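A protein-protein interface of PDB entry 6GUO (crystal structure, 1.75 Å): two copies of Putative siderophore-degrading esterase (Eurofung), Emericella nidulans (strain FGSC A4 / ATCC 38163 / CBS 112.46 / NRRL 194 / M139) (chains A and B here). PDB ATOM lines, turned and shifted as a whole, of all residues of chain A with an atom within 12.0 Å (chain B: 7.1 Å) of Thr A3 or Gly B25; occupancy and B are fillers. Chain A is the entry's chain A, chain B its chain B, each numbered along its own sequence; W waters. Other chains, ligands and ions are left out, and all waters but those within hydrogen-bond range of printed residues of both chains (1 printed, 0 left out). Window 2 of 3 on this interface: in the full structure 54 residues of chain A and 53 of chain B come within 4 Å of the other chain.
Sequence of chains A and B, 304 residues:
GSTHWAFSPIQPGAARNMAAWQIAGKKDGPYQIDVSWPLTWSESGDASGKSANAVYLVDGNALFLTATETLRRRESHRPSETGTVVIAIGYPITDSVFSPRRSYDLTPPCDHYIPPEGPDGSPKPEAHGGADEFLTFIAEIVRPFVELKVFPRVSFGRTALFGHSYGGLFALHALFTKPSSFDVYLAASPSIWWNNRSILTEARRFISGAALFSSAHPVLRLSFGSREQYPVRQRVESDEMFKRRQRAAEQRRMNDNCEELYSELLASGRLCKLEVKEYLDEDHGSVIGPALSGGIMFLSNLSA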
ATOM      1  N   THR A   3      14.069 -15.127 -34.730  1.00  0.00           N
ATOM      2  CA  THR A   3      13.404 -15.475 -33.433  1.00  0.00           C
ATOM      3  C   THR A   3      14.353 -15.266 -32.250  1.00  0.00           C
ATOM      4  O   THR A   3      15.486 -15.755 -32.253  1.00  0.00           O
ATOM      5  CB  THR A   3      12.894 -16.937 -33.420  1.00  0.00           C
ATOM      6  OG1 THR A   3      12.087 -17.175 -34.579  1.00  0.00           O
ATOM      7  CG2 THR A   3      12.058 -17.229 -32.163  1.00  0.00           C
ATOM      8  N   HIS A   4      13.869 -14.550 -31.239  1.00  0.00           N
ATOM      9  CA  HIS A   4      14.644 -14.274 -30.034  1.00  0.00           C
ATOM     10  C   HIS A   4      14.579 -15.471 -29.080  1.00  0.00           C
ATOM     11  O   HIS A   4      13.855 -15.443 -28.077  1.00  0.00           O
ATOM     12  CB  HIS A   4      14.140 -12.982 -29.373  1.00  0.00           C
ATOM     13  CG  HIS A   4      14.297 -11.768 -30.238  1.00  0.00           C
ATOM     14  ND1 HIS A   4      15.524 -11.338 -30.699  1.00  0.00           N
ATOM     15  CD2 HIS A   4      13.384 -10.901 -30.736  1.00  0.00           C
ATOM     16  CE1 HIS A   4      15.359 -10.256 -31.440  1.00  0.00           C
ATOM     17  NE2 HIS A   4      14.070  -9.970 -31.476  1.00  0.00           N
ATOM     18  N   TRP A   5      15.335 -16.522 -29.412  1.00  0.00           N
ATOM     19  CA  TRP A   5      15.396 -17.738 -28.587  1.00  0.00           C
ATOM     20  C   TRP A   5      16.193 -17.466 -27.321  1.00  0.00           C
ATOM     21  O   TRP A   5      17.294 -16.918 -27.387  1.00  0.00           O
ATOM     22  CB  TRP A   5      16.048 -18.909 -29.329  1.00  0.00           C
ATOM     23  CG  TRP A   5      15.228 -19.472 -30.439  1.00  0.00           C
ATOM     24  CD1 TRP A   5      15.552 -19.487 -31.764  1.00  0.00           C
ATOM     25  CD2 TRP A   5      13.951 -20.112 -30.330  1.00  0.00           C
ATOM     26  NE1 TRP A   5      14.556 -20.092 -32.489  1.00  0.00           N
ATOM     27  CE2 TRP A   5      13.559 -20.483 -31.635  1.00  0.00           C
ATOM     28  CE3 TRP A   5      13.095 -20.399 -29.260  1.00  0.00           C
ATOM     29  CZ2 TRP A   5      12.348 -21.135 -31.899  1.00  0.00           C
ATOM     30  CZ3 TRP A   5      11.887 -21.048 -29.523  1.00  0.00           C
ATOM     31  CH2 TRP A   5      11.528 -21.407 -30.833  1.00  0.00           C
ATOM     32  N   ALA A   6      15.628 -17.850 -26.181  1.00  0.00           N
ATOM     33  CA  ALA A   6      16.271 -17.688 -24.882  1.00  0.00           C
ATOM     34  C   ALA A   6      16.169 -19.002 -24.136  1.00  0.00           C
ATOM     35  O   ALA A   6      15.080 -19.549 -24.021  1.00  0.00           O
ATOM     36  CB  ALA A   6      15.574 -16.596 -24.093  1.00  0.00           C
ATOM     37  N   PHE A   7      17.301 -19.509 -23.656  1.00  0.00           N
ATOM     38  CA  PHE A   7      17.339 -20.677 -22.778  1.00  0.00           C
ATOM     39  C   PHE A   7      17.663 -20.172 -21.377  1.00  0.00           C
ATOM     40  O   PHE A   7      18.824 -19.921 -21.055  1.00  0.00           O
ATOM     41  CB  PHE A   7      18.391 -21.674 -23.255  1.00  0.00           C
ATOM     42  CG  PHE A   7      18.070 -22.292 -24.582  1.00  0.00           C
ATOM     43  CD1 PHE A   7      17.503 -23.560 -24.657  1.00  0.00           C
ATOM     44  CD2 PHE A   7      18.327 -21.602 -25.761  1.00  0.00           C
ATOM     45  CE1 PHE A   7      17.204 -24.130 -25.888  1.00  0.00           C
ATOM     46  CE2 PHE A   7      18.026 -22.166 -26.993  1.00  0.00           C
ATOM     47  CZ  PHE A   7      17.466 -23.434 -27.054  1.00  0.00           C
ATOM     48  N   SER A   8      16.622 -19.997 -20.568  1.00  0.00           N
ATOM     49  CA  SER A   8      16.738 -19.399 -19.240  1.00  0.00           C
ATOM     50  C   SER A   8      16.678 -20.496 -18.176  1.00  0.00           C
ATOM     51  O   SER A   8      15.651 -21.157 -18.060  1.00  0.00           O
ATOM     52  CB  SER A   8      15.594 -18.402 -19.019  1.00  0.00           C
ATOM     53  OG  SER A   8      15.497 -17.483 -20.097  1.00  0.00           O
ATOM     54  N   ILE B  23      12.364 -22.085 -22.352  1.00  0.00           N
ATOM     55  CA  ILE B  23      12.742 -21.700 -23.705  1.00  0.00           C
ATOM     56  C   ILE B  23      11.662 -20.753 -24.215  1.00  0.00           C
ATOM     57  O   ILE B  23      10.535 -21.175 -24.475  1.00  0.00           O
ATOM     58  CB  ILE B  23      12.922 -22.917 -24.639  1.00  0.00           C
ATOM     59  CG1 ILE B  23      13.917 -23.911 -24.021  1.00  0.00           C
ATOM     60  CG2 ILE B  23      13.414 -22.463 -26.010  1.00  0.00           C
ATOM     61  CD1 ILE B  23      14.070 -25.213 -24.777  1.00  0.00           C
ATOM     62  N   ALA B  24      12.019 -19.475 -24.331  1.00  0.00           N
ATOM     63  CA  ALA B  24      11.127 -18.430 -24.829  1.00  0.00           C
ATOM     64  C   ALA B  24      11.478 -18.098 -26.270  1.00  0.00           C
ATOM     65  O   ALA B  24      12.627 -18.263 -26.682  1.00  0.00           O
ATOM     66  CB  ALA B  24      11.251 -17.188 -23.962  1.00  0.00           C
ATOM     67  N   GLY B  25      10.488 -17.630 -27.029  1.00  0.00           N
ATOM     68  CA  GLY B  25      10.681 -17.229 -28.425  1.00  0.00           C
ATOM     69  C   GLY B  25       9.538 -17.607 -29.348  1.00  0.00           C
ATOM     70  O   GLY B  25       9.200 -16.846 -30.258  1.00  0.00           O
ATOM     71  N   LYS B  26       8.943 -18.780 -29.120  1.00  0.00           N
ATOM     72  CA  LYS B  26       7.907 -19.304 -30.015  1.00  0.00           C
ATOM     73  C   LYS B  26       6.578 -18.561 -29.847  1.00  0.00           C
ATOM     74  O   LYS B  26       6.275 -18.042 -28.769  1.00  0.00           O
ATOM     75  CB  LYS B  26       7.707 -20.812 -29.805  1.00  0.00           C
ATOM     76  CG  LYS B  26       7.171 -21.538 -31.029  1.00  0.00           C
ATOM     77  CD  LYS B  26       6.992 -23.016 -30.747  1.00  0.00           C
ATOM     78  CE  LYS B  26       6.839 -23.844 -32.007  1.00  0.00           C
ATOM     79  NZ  LYS B  26       6.495 -25.248 -31.650  1.00  0.00           N
ATOM     80  N   LYS B  27       5.814 -18.518 -30.939  1.00  0.00           N
ATOM     81  CA  LYS B  27       4.504 -17.850 -31.024  1.00  0.00           C
ATOM     82  C   LYS B  27       3.571 -18.116 -29.837  1.00  0.00           C
ATOM     83  O   LYS B  27       3.020 -17.179 -29.253  1.00  0.00           O
ATOM     84  CB  LYS B  27       3.816 -18.283 -32.333  1.00  0.00           C
ATOM     85  CG  LYS B  27       2.391 -17.791 -32.559  1.00  0.00           C
ATOM     86  CD  LYS B  27       2.294 -16.274 -32.519  1.00  0.00           C
ATOM     87  CE  LYS B  27       1.029 -15.774 -33.200  1.00  0.00           C
ATOM     88  NZ  LYS B  27       1.059 -14.300 -33.408  1.00  0.00           N
ATOM     89  N   ASP B  28       3.411 -19.390 -29.490  1.00  0.00           N
ATOM     90  CA  ASP B  28       2.412 -19.819 -28.500  1.00  0.00           C
ATOM     91  C   ASP B  28       2.762 -19.484 -27.045  1.00  0.00           C
ATOM     92  O   ASP B  28       1.874 -19.471 -26.189  1.00  0.00           O
ATOM     93  CB  ASP B  28       2.162 -21.326 -28.621  1.00  0.00           C
ATOM     94  CG  ASP B  28       1.632 -21.724 -29.988  1.00  0.00           C
ATOM     95  OD1 ASP B  28       2.298 -22.534 -30.669  1.00  0.00           O
ATOM     96  OD2 ASP B  28       0.559 -21.220 -30.383  1.00  0.00           O
ATOM     97  N   GLY B  29       4.042 -19.226 -26.769  1.00  0.00           N
ATOM     98  CA  GLY B  29       4.525 -18.941 -25.416  1.00  0.00           C
ATOM     99  C   GLY B  29       5.745 -19.785 -25.091  1.00  0.00           C
ATOM    100  O   GLY B  29       6.174 -20.595 -25.916  1.00  0.00           O
ATOM    101  N   PRO B  30       6.312 -19.611 -23.882  1.00  0.00           N
ATOM    102  CA  PRO B  30       7.526 -20.350 -23.540  1.00  0.00           C
ATOM    103  C   PRO B  30       7.279 -21.842 -23.307  1.00  0.00           C
ATOM    104  O   PRO B  30       6.167 -22.238 -22.952  1.00  0.00           O
ATOM    105  CB  PRO B  30       8.009 -19.684 -22.238  1.00  0.00           C
ATOM    106  CG  PRO B  30       7.083 -18.545 -21.972  1.00  0.00           C
ATOM    107  CD  PRO B  30       5.835 -18.794 -22.755  1.00  0.00           C
ATOM    108  N   TYR B  31       8.319 -22.644 -23.519  1.00  0.00           N
ATOM    109  CA  TYR B  31       8.329 -24.054 -23.137  1.00  0.00           C
ATOM    110  C   TYR B  31       9.228 -24.238 -21.924  1.00  0.00           C
ATOM    111  O   TYR B  31      10.124 -23.433 -21.682  1.00  0.00           O
ATOM    112  CB  TYR B  31       8.821 -24.927 -24.294  1.00  0.00           C
ATOM    113  CG  TYR B  31       7.825 -25.016 -25.418  1.00  0.00           C
ATOM    114  CD1 TYR B  31       6.889 -26.049 -25.470  1.00  0.00           C
ATOM    115  CD2 TYR B  31       7.796 -24.054 -26.419  1.00  0.00           C
ATOM    116  CE1 TYR B  31       5.959 -26.123 -26.498  1.00  0.00           C
ATOM    117  CE2 TYR B  31       6.876 -24.124 -27.453  1.00  0.00           C
ATOM    118  CZ  TYR B  31       5.960 -25.157 -27.490  1.00  0.00           C
ATOM    119  OH  TYR B  31       5.043 -25.226 -28.516  1.00  0.00           O
HETATM  120  O   HOH W   1      13.186 -18.267 -21.594  1.00  0.00           O
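Thr A3 touches one residue of chain B.
Of the printed residues of chain B, His A4 touches Ala B24 (3.4 Å) and Gly B25 (3.7 Å).
Printed residues of chain B within 4 Å of Trp A5: Ile B23, Ala B24 and Lys B26.
Printed residues of chain B within 4 Å of Ala A6: Ile B23 (3.2 Å) and Ala B24 (3.1 Å).
Of the printed residues of chain B, Phe A7 touches Ile B23.
Printed residues of chain A within 4 Å of Gly B25: Thr A3 and His A4.
No residue of chain A comes within 4 Å of Gly B29.
No residue of chain A comes within 4 Å of Pro B30.
The nearest residue of chain B that does not touch Thr A3 is Lys B26 (4.6 Å).
The nearest residue of chain A that does not touch Gly B25 is Trp A5 (4.1 Å).
The nearest printed residue of chain B that does not touch Trp A5 is Gly B25 (4.1 Å).
The backbone NH (N) of Ile B23 lies within hydrogen-bond range of the backbone carbonyl oxygen (O) of Tyr B31 (2.7 Å).
The side-chain amino group (NZ) of Lys B26 is in hydrogen-bond range of the side-chain hydroxyl (OH) of Tyr B31 (3.5 Å).
Water W1 lies within hydrogen-bond range of OG of Ser A8 (2.9 Å), N of Ala B24 (3.2 Å) and O of Ala A6 (3.3 Å).
Among the printed residues, pairs that only touch across the chains: Ala A6 with Ile B23 (3.2 Å), Trp A5 with Ala B24 (3.4 Å), Thr A3 with Gly B25 (3.5 Å), Phe A7 with Ile B23 (3.5 Å), His A4 with Gly B25 (3.7 Å), Trp A5 with Lys B26 (3.7 Å) and Trp A5 with Ile B23 (3.9 Å).
No position is printed for both chains.
Of the 9 pairs that touch across the chains among the printed residues, none has its exchanged pair printed and touching as well.
N of Ala A6 lies within hydrogen-bond range of O of Ala B24 (3.1 Å).
O of Ala B24 sits close to O of His A4 (3.4 Å).
Of the 9 printed residues of chain B, 4 touch a printed residue of chain A.
Hydrophobic or aromatic side chains of chain B within 4 Å of the printed part of chain A: Ile B23.
Hydrophobic or aromatic side chains of chain A that line the printed part of chain B: Trp A5 and Phe A7.
Among the printed residues, no Asp or Glu carboxylate lies within 4 Å of a Lys or Arg side-chain nitrogen of the other chain.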
